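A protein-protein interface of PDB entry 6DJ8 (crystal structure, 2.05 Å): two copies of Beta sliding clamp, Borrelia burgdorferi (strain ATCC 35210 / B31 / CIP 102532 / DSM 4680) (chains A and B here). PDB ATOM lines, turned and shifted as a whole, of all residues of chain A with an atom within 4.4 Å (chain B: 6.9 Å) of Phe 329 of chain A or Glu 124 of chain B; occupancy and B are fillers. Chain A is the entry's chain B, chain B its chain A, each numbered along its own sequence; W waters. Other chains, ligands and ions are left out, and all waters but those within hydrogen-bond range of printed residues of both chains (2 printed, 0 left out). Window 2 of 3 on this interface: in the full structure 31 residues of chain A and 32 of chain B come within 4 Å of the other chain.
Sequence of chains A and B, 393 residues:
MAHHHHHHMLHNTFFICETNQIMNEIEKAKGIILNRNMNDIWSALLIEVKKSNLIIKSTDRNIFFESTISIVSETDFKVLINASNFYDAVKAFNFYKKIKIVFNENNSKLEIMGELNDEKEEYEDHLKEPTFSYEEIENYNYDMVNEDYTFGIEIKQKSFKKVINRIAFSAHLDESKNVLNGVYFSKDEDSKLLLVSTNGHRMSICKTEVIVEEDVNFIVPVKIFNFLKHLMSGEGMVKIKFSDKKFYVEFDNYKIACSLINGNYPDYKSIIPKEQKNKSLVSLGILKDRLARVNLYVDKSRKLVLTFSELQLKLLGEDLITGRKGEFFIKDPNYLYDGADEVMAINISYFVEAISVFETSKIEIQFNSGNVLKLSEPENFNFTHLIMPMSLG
The side-chain carboxylate (OD1) of Asp 125 of chain B sits at hydrogen-bond distance from the backbone NH (N) of Phe 329 of chain A (2.8 Å).
The side-chain amino group of Lys 331 of chain A sits at hydrogen-bond distance from the backbone carbonyl oxygen of Tyr 123 of chain B, 2.7 Å away.
The side-chain carboxylate (OE1) of Glu 121 of chain B is in salt-bridge range of the side-chain amino group (NZ) of Lys 331 of chain A (2.9 Å).
The side-chain hydroxyl (OH) of Tyr 96 of chain B lies within hydrogen-bond range of the side-chain carboxylate (OD2) of Asp 125 of chain B.
N of Glu 121 of chain B is in hydrogen-bond range of OE1 of Glu 124 of chain B (2.8 Å).
Among the printed residues, merely in contact across the chains: Gln 312 of chain A with Tyr 123 of chain B (3.1 Å), Phe 329 of chain A with Glu 124 of chain B (3.3 Å), Phe 328 of chain A with Asp 125 of chain B (3.3 Å), Phe 328 of chain A with Phe 93 of chain B (3.5 Å), Phe 329 of chain A with Tyr 123 of chain B (3.6 Å) and Phe 328 of chain A with Leu 127 of chain B (3.8 Å).
Of chain B, only Tyr 123, Glu 124 and Asp 125 come within 4 Å of Phe 329 of chain A.
Of the printed residues of chain A, Asp 125 of chain B touches Phe 328 and Phe 329.
Printed residues of chain B within 4 Å of Gln 312 of chain A: Tyr 123 (3.1 Å).
The nearest printed residue of chain A that does not touch Glu 124 of chain B is Lys 331 of chain A (4.6 Å).
The nearest printed residue of chain A that does not touch Asp 125 of chain B is Ile 330 of chain A (5.7 Å).
Hydrophobic or aromatic side chains of chain B that line the printed part of chain A: Phe 93, Tyr 123 and Leu 127.
Printed residues of chain A that touch a printed residue of chain B: Gln 312, Phe 328, Phe 329 and Lys 331.
Hydrophobic or aromatic side chains of chain A that line the printed part of chain B: Phe 328 and Phe 329.
No position is printed for both chains.
Of the 9 pairs that touch across the chains among the printed residues, none has its exchanged pair printed and touching as well.
Water W2 lies within hydrogen-bond range of OD2 of Asp 125 of chain B (2.7 Å) and O of Phe 329 of chain A (2.8 Å).
Water W1 bridges the side-chain carboxylate of Asp 125 of chain B (3.1 Å) and the backbone carbonyl oxygen of Phe 329 of chain A (3.3 Å).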
ATOM      1  N   GLN A 312      16.256  -4.173  11.933  1.00  0.00           N
ATOM      2  CA  GLN A 312      16.139  -4.494  13.351  1.00  0.00           C
ATOM      3  C   GLN A 312      17.304  -5.347  13.828  1.00  0.00           C
ATOM      4  O   GLN A 312      18.003  -5.996  13.045  1.00  0.00           O
ATOM      5  CB  GLN A 312      14.825  -5.228  13.653  1.00  0.00           C
ATOM      6  CG  GLN A 312      14.818  -6.684  13.205  1.00  0.00           C
ATOM      7  CD  GLN A 312      13.427  -7.194  12.865  1.00  0.00           C
ATOM      8  OE1 GLN A 312      12.524  -6.414  12.567  1.00  0.00           O
ATOM      9  NE2 GLN A 312      13.252  -8.512  12.903  1.00  0.00           N
ATOM     10  N   LEU A 313      17.498  -5.314  15.147  1.00  0.00           N
ATOM     11  CA  LEU A 313      18.365  -6.226  15.877  1.00  0.00           C
ATOM     12  C   LEU A 313      17.494  -7.163  16.699  1.00  0.00           C
ATOM     13  O   LEU A 313      16.611  -6.708  17.440  1.00  0.00           O
ATOM     14  CB  LEU A 313      19.314  -5.466  16.805  1.00  0.00           C
ATOM     15  CG  LEU A 313      20.071  -6.346  17.804  1.00  0.00           C
ATOM     16  CD1 LEU A 313      20.958  -7.321  17.049  1.00  0.00           C
ATOM     17  CD2 LEU A 313      20.892  -5.536  18.815  1.00  0.00           C
ATOM     18  N   LYS A 314      17.727  -8.462  16.566  1.00  0.00           N
ATOM     19  CA  LYS A 314      16.971  -9.455  17.315  1.00  0.00           C
ATOM     20  C   LYS A 314      17.851 -10.066  18.400  1.00  0.00           C
ATOM     21  O   LYS A 314      19.007 -10.418  18.145  1.00  0.00           O
ATOM     22  CB  LYS A 314      16.426 -10.542  16.389  1.00  0.00           C
ATOM     23  CG  LYS A 314      15.687 -11.650  17.131  1.00  0.00           C
ATOM     24  CD  LYS A 314      15.270 -12.765  16.175  1.00  0.00           C
ATOM     25  CE  LYS A 314      14.312 -13.714  16.871  1.00  0.00           C
ATOM     26  NZ  LYS A 314      14.292 -15.040  16.202  1.00  0.00           N
ATOM     27  N   PHE A 328      13.393 -10.593  21.734  1.00  0.00           N
ATOM     28  CA  PHE A 328      13.219  -9.147  21.779  1.00  0.00           C
ATOM     29  C   PHE A 328      13.823  -8.497  20.537  1.00  0.00           C
ATOM     30  O   PHE A 328      14.844  -8.950  20.009  1.00  0.00           O
ATOM     31  CB  PHE A 328      13.861  -8.574  23.031  1.00  0.00           C
ATOM     32  CG  PHE A 328      13.230  -9.081  24.307  1.00  0.00           C
ATOM     33  CD1 PHE A 328      13.562 -10.324  24.816  1.00  0.00           C
ATOM     34  CD2 PHE A 328      12.326  -8.300  24.997  1.00  0.00           C
ATOM     35  CE1 PHE A 328      12.971 -10.791  26.000  1.00  0.00           C
ATOM     36  CE2 PHE A 328      11.731  -8.757  26.173  1.00  0.00           C
ATOM     37  CZ  PHE A 328      12.061  -9.998  26.669  1.00  0.00           C
ATOM     38  N   PHE A 329      13.189  -7.421  20.076  1.00  0.00           N
ATOM     39  CA  PHE A 329      13.625  -6.718  18.876  1.00  0.00           C
ATOM     40  C   PHE A 329      13.913  -5.259  19.199  1.00  0.00           C
ATOM     41  O   PHE A 329      13.206  -4.639  19.999  1.00  0.00           O
ATOM     42  CB  PHE A 329      12.571  -6.786  17.771  1.00  0.00           C
ATOM     43  CG  PHE A 329      12.275  -8.178  17.294  1.00  0.00           C
ATOM     44  CD1 PHE A 329      11.294  -8.952  17.918  1.00  0.00           C
ATOM     45  CD2 PHE A 329      12.968  -8.712  16.214  1.00  0.00           C
ATOM     46  CE1 PHE A 329      11.007 -10.239  17.474  1.00  0.00           C
ATOM     47  CE2 PHE A 329      12.690 -10.003  15.754  1.00  0.00           C
ATOM     48  CZ  PHE A 329      11.709 -10.769  16.387  1.00  0.00           C
ATOM     49  N   ILE A 330      14.939  -4.705  18.565  1.00  0.00           N
ATOM     50  CA  ILE A 330      15.258  -3.284  18.659  1.00  0.00           C
ATOM     51  C   ILE A 330      15.225  -2.736  17.244  1.00  0.00           C
ATOM     52  O   ILE A 330      15.874  -3.290  16.348  1.00  0.00           O
ATOM     53  CB  ILE A 330      16.629  -3.054  19.327  1.00  0.00           C
ATOM     54  CG1 ILE A 330      16.636  -3.633  20.740  1.00  0.00           C
ATOM     55  CG2 ILE A 330      16.996  -1.558  19.386  1.00  0.00           C
ATOM     56  CD1 ILE A 330      17.979  -3.518  21.449  1.00  0.00           C
ATOM     57  N   LYS A 331      14.438  -1.683  17.029  1.00  0.00           N
ATOM     58  CA  LYS A 331      14.206  -1.201  15.677  1.00  0.00           C
ATOM     59  C   LYS A 331      14.420   0.301  15.624  1.00  0.00           C
ATOM     60  O   LYS A 331      14.589   0.965  16.652  1.00  0.00           O
ATOM     61  CB  LYS A 331      12.778  -1.508  15.209  1.00  0.00           C
ATOM     62  CG  LYS A 331      12.355  -2.956  15.334  1.00  0.00           C
ATOM     63  CD  LYS A 331      10.867  -3.089  15.048  1.00  0.00           C
ATOM     64  CE  LYS A 331      10.411  -4.532  15.111  1.00  0.00           C
ATOM     65  NZ  LYS A 331       8.945  -4.634  14.933  1.00  0.00           N
ATOM     66  N   PHE B  93       8.437  -8.590  30.619  1.00  0.00           N
ATOM     67  CA  PHE B  93       7.527  -7.749  29.862  1.00  0.00           C
ATOM     68  C   PHE B  93       6.957  -6.585  30.682  1.00  0.00           C
ATOM     69  O   PHE B  93       5.922  -6.026  30.312  1.00  0.00           O
ATOM     70  CB  PHE B  93       6.406  -8.618  29.273  1.00  0.00           C
ATOM     71  CG  PHE B  93       6.732  -9.170  27.885  1.00  0.00           C
ATOM     72  CD1 PHE B  93       8.015  -9.061  27.360  1.00  0.00           C
ATOM     73  CD2 PHE B  93       5.752  -9.786  27.111  1.00  0.00           C
ATOM     74  CE1 PHE B  93       8.318  -9.554  26.082  1.00  0.00           C
ATOM     75  CE2 PHE B  93       6.045 -10.283  25.826  1.00  0.00           C
ATOM     76  CZ  PHE B  93       7.335 -10.167  25.311  1.00  0.00           C
ATOM     77  N   TYR B  96       5.367  -3.305  29.138  1.00  0.00           N
ATOM     78  CA  TYR B  96       4.018  -3.248  28.588  1.00  0.00           C
ATOM     79  C   TYR B  96       3.016  -2.970  29.698  1.00  0.00           C
ATOM     80  O   TYR B  96       3.084  -3.574  30.775  1.00  0.00           O
ATOM     81  CB  TYR B  96       3.623  -4.555  27.908  1.00  0.00           C
ATOM     82  CG  TYR B  96       4.387  -4.850  26.647  1.00  0.00           C
ATOM     83  CD1 TYR B  96       4.291  -4.020  25.534  1.00  0.00           C
ATOM     84  CD2 TYR B  96       5.202  -5.961  26.569  1.00  0.00           C
ATOM     85  CE1 TYR B  96       4.991  -4.302  24.372  1.00  0.00           C
ATOM     86  CE2 TYR B  96       5.903  -6.245  25.422  1.00  0.00           C
ATOM     87  CZ  TYR B  96       5.795  -5.412  24.334  1.00  0.00           C
ATOM     88  OH  TYR B  96       6.493  -5.721  23.212  1.00  0.00           O
ATOM     89  N   MET B 113       2.743 -12.049  24.727  1.00  0.00           N
ATOM     90  CA  MET B 113       3.061 -10.933  23.865  1.00  0.00           C
ATOM     91  C   MET B 113       2.484  -9.700  24.527  1.00  0.00           C
ATOM     92  O   MET B 113       1.582  -9.792  25.372  1.00  0.00           O
ATOM     93  CB  MET B 113       2.495 -11.142  22.446  1.00  0.00           C
ATOM     94  CG  MET B 113       0.972 -11.306  22.428  1.00  0.00           C
ATOM     95  SD  MET B 113       0.394 -12.639  21.341  1.00  0.00           S
ATOM     96  CE  MET B 113       1.214 -14.046  22.100  1.00  0.00           C
ATOM     97  N   GLY B 114       3.023  -8.539  24.174  1.00  0.00           N
ATOM     98  CA  GLY B 114       2.435  -7.311  24.669  1.00  0.00           C
ATOM     99  C   GLY B 114       1.073  -7.128  24.040  1.00  0.00           C
ATOM    100  O   GLY B 114       0.889  -7.393  22.845  1.00  0.00           O
ATOM    101  N   LEU B 116      -0.712  -4.666  22.793  1.00  0.00           N
ATOM    102  CA  LEU B 116      -0.634  -3.300  22.321  1.00  0.00           C
ATOM    103  C   LEU B 116      -2.026  -2.809  21.951  1.00  0.00           C
ATOM    104  O   LEU B 116      -2.994  -3.575  21.894  1.00  0.00           O
ATOM    105  CB  LEU B 116       0.316  -3.219  21.134  1.00  0.00           C
ATOM    106  CG  LEU B 116       1.570  -4.045  21.413  1.00  0.00           C
ATOM    107  CD1 LEU B 116       2.218  -4.557  20.127  1.00  0.00           C
ATOM    108  CD2 LEU B 116       2.542  -3.213  22.222  1.00  0.00           C
ATOM    109  N   ASP B 118      -2.838  -1.177  18.979  1.00  0.00           N
ATOM    110  CA  ASP B 118      -3.262  -1.569  17.636  1.00  0.00           C
ATOM    111  C   ASP B 118      -2.266  -2.526  16.976  1.00  0.00           C
ATOM    112  O   ASP B 118      -1.555  -3.255  17.677  1.00  0.00           O
ATOM    113  CB  ASP B 118      -3.610  -0.313  16.797  1.00  0.00           C
ATOM    114  CG  ASP B 118      -2.431   0.316  16.075  1.00  0.00           C
ATOM    115  OD1 ASP B 118      -1.994  -0.255  15.062  1.00  0.00           O
ATOM    116  OD2 ASP B 118      -2.006   1.420  16.463  1.00  0.00           O
ATOM    117  N   GLU B 119      -2.233  -2.545  15.643  1.00  0.00           N
ATOM    118  CA  GLU B 119      -1.783  -3.694  14.860  1.00  0.00           C
ATOM    119  C   GLU B 119      -0.436  -4.243  15.317  1.00  0.00           C
ATOM    120  O   GLU B 119       0.457  -3.496  15.725  1.00  0.00           O
ATOM    121  CB  GLU B 119      -1.694  -3.298  13.384  1.00  0.00           C
ATOM    122  CG  GLU B 119      -1.915  -4.431  12.411  1.00  0.00           C
ATOM    123  CD  GLU B 119      -3.320  -4.447  11.852  1.00  0.00           C
ATOM    124  OE1 GLU B 119      -4.061  -5.403  12.143  1.00  0.00           O
ATOM    125  OE2 GLU B 119      -3.690  -3.500  11.129  1.00  0.00           O
ATOM    126  N   LYS B 120      -0.292  -5.565  15.219  1.00  0.00           N
ATOM    127  CA  LYS B 120       0.988  -6.226  15.430  1.00  0.00           C
ATOM    128  C   LYS B 120       1.765  -6.262  14.123  1.00  0.00           C
ATOM    129  O   LYS B 120       1.188  -6.440  13.048  1.00  0.00           O
ATOM    130  CB  LYS B 120       0.796  -7.645  15.961  1.00  0.00           C
ATOM    131  CG  LYS B 120       0.121  -7.706  17.320  1.00  0.00           C
ATOM    132  CD  LYS B 120       0.233  -9.091  17.939  1.00  0.00           C
ATOM    133  CE  LYS B 120      -0.376  -9.118  19.327  1.00  0.00           C
ATOM    134  NZ  LYS B 120       0.136  -7.982  20.144  1.00  0.00           N
ATOM    135  N   GLU B 121       3.074  -6.066  14.218  1.00  0.00           N
ATOM    136  CA  GLU B 121       3.945  -6.154  13.058  1.00  0.00           C
ATOM    137  C   GLU B 121       4.398  -7.603  12.876  1.00  0.00           C
ATOM    138  O   GLU B 121       4.030  -8.500  13.641  1.00  0.00           O
ATOM    139  CB  GLU B 121       5.138  -5.211  13.210  1.00  0.00           C
ATOM    140  CG  GLU B 121       4.781  -3.726  13.292  1.00  0.00           C
ATOM    141  CD  GLU B 121       6.002  -2.836  13.520  1.00  0.00           C
ATOM    142  OE1 GLU B 121       6.602  -2.916  14.611  1.00  0.00           O
ATOM    143  OE2 GLU B 121       6.369  -2.061  12.608  1.00  0.00           O
ATOM    144  N   GLU B 122       5.218  -7.833  11.849  1.00  0.00           N
ATOM    145  CA  GLU B 122       5.779  -9.164  11.635  1.00  0.00           C
ATOM    146  C   GLU B 122       6.610  -9.610  12.834  1.00  0.00           C
ATOM    147  O   GLU B 122       6.506 -10.758  13.281  1.00  0.00           O
ATOM    148  CB  GLU B 122       6.629  -9.177  10.362  1.00  0.00           C
ATOM    149  N   TYR B 123       7.421  -8.713  13.379  1.00  0.00           N
ATOM    150  CA  TYR B 123       8.406  -9.048  14.405  1.00  0.00           C
ATOM    151  C   TYR B 123       8.069  -8.291  15.687  1.00  0.00           C
ATOM    152  O   TYR B 123       8.267  -7.076  15.772  1.00  0.00           O
ATOM    153  CB  TYR B 123       9.815  -8.745  13.914  1.00  0.00           C
ATOM    154  CG  TYR B 123      10.236  -9.617  12.734  1.00  0.00           C
ATOM    155  CD1 TYR B 123      10.305 -11.005  12.859  1.00  0.00           C
ATOM    156  CD2 TYR B 123      10.555  -9.056  11.503  1.00  0.00           C
ATOM    157  CE1 TYR B 123      10.688 -11.811  11.789  1.00  0.00           C
ATOM    158  CE2 TYR B 123      10.940  -9.859  10.424  1.00  0.00           C
ATOM    159  CZ  TYR B 123      10.998 -11.234  10.580  1.00  0.00           C
ATOM    160  OH  TYR B 123      11.376 -12.034   9.525  1.00  0.00           O
ATOM    161  N   GLU B 124       7.514  -8.998  16.664  1.00  0.00           N
ATOM    162  CA  GLU B 124       7.162  -8.440  17.958  1.00  0.00           C
ATOM    163  C   GLU B 124       7.831  -9.263  19.049  1.00  0.00           C
ATOM    164  O   GLU B 124       8.078 -10.460  18.878  1.00  0.00           O
ATOM    165  CB  GLU B 124       5.632  -8.461  18.184  1.00  0.00           C
ATOM    166  CG  GLU B 124       4.794  -7.661  17.187  1.00  0.00           C
ATOM    167  CD  GLU B 124       4.976  -6.151  17.346  1.00  0.00           C
ATOM    168  OE1 GLU B 124       4.698  -5.397  16.383  1.00  0.00           O
ATOM    169  OE2 GLU B 124       5.383  -5.716  18.446  1.00  0.00           O
ATOM    170  N   ASP B 125       8.101  -8.627  20.184  1.00  0.00           N
ATOM    171  CA  ASP B 125       8.674  -9.353  21.308  1.00  0.00           C
ATOM    172  C   ASP B 125       7.739 -10.485  21.731  1.00  0.00           C
ATOM    173  O   ASP B 125       6.513 -10.350  21.700  1.00  0.00           O
ATOM    174  CB  ASP B 125       8.931  -8.410  22.487  1.00  0.00           C
ATOM    175  CG  ASP B 125       9.829  -7.238  22.116  1.00  0.00           C
ATOM    176  OD1 ASP B 125      10.563  -7.339  21.110  1.00  0.00           O
ATOM    177  OD2 ASP B 125       9.801  -6.216  22.836  1.00  0.00           O
ATOM    178  N   HIS B 126       8.326 -11.609  22.130  1.00  0.00           N
ATOM    179  CA  HIS B 126       7.561 -12.823  22.346  1.00  0.00           C
ATOM    180  C   HIS B 126       8.284 -13.710  23.344  1.00  0.00           C
ATOM    181  O   HIS B 126       9.506 -13.856  23.280  1.00  0.00           O
ATOM    182  CB  HIS B 126       7.356 -13.571  21.020  1.00  0.00           C
ATOM    183  CG  HIS B 126       6.358 -14.683  21.097  1.00  0.00           C
ATOM    184  ND1 HIS B 126       5.016 -14.504  20.832  1.00  0.00           N
ATOM    185  CD2 HIS B 126       6.510 -15.995  21.392  1.00  0.00           C
ATOM    186  CE1 HIS B 126       4.386 -15.658  20.962  1.00  0.00           C
ATOM    187  NE2 HIS B 126       5.269 -16.578  21.303  1.00  0.00           N
ATOM    188  N   LEU B 127       7.520 -14.298  24.262  1.00  0.00           N
ATOM    189  CA  LEU B 127       8.032 -15.238  25.249  1.00  0.00           C
ATOM    190  C   LEU B 127       7.272 -16.548  25.124  1.00  0.00           C
ATOM    191  O   LEU B 127       6.075 -16.558  24.837  1.00  0.00           O
ATOM    192  CB  LEU B 127       7.863 -14.713  26.675  1.00  0.00           C
ATOM    193  CG  LEU B 127       8.186 -13.249  26.965  1.00  0.00           C
ATOM    194  CD1 LEU B 127       7.823 -12.887  28.422  1.00  0.00           C
ATOM    195  CD2 LEU B 127       9.679 -12.948  26.690  1.00  0.00           C
HETATM  196  O   HOH W   1       9.920  -4.782  19.549  1.00  0.00           O
HETATM  197  O   HOH W   2      12.244  -5.168  22.545  1.00  0.00           O
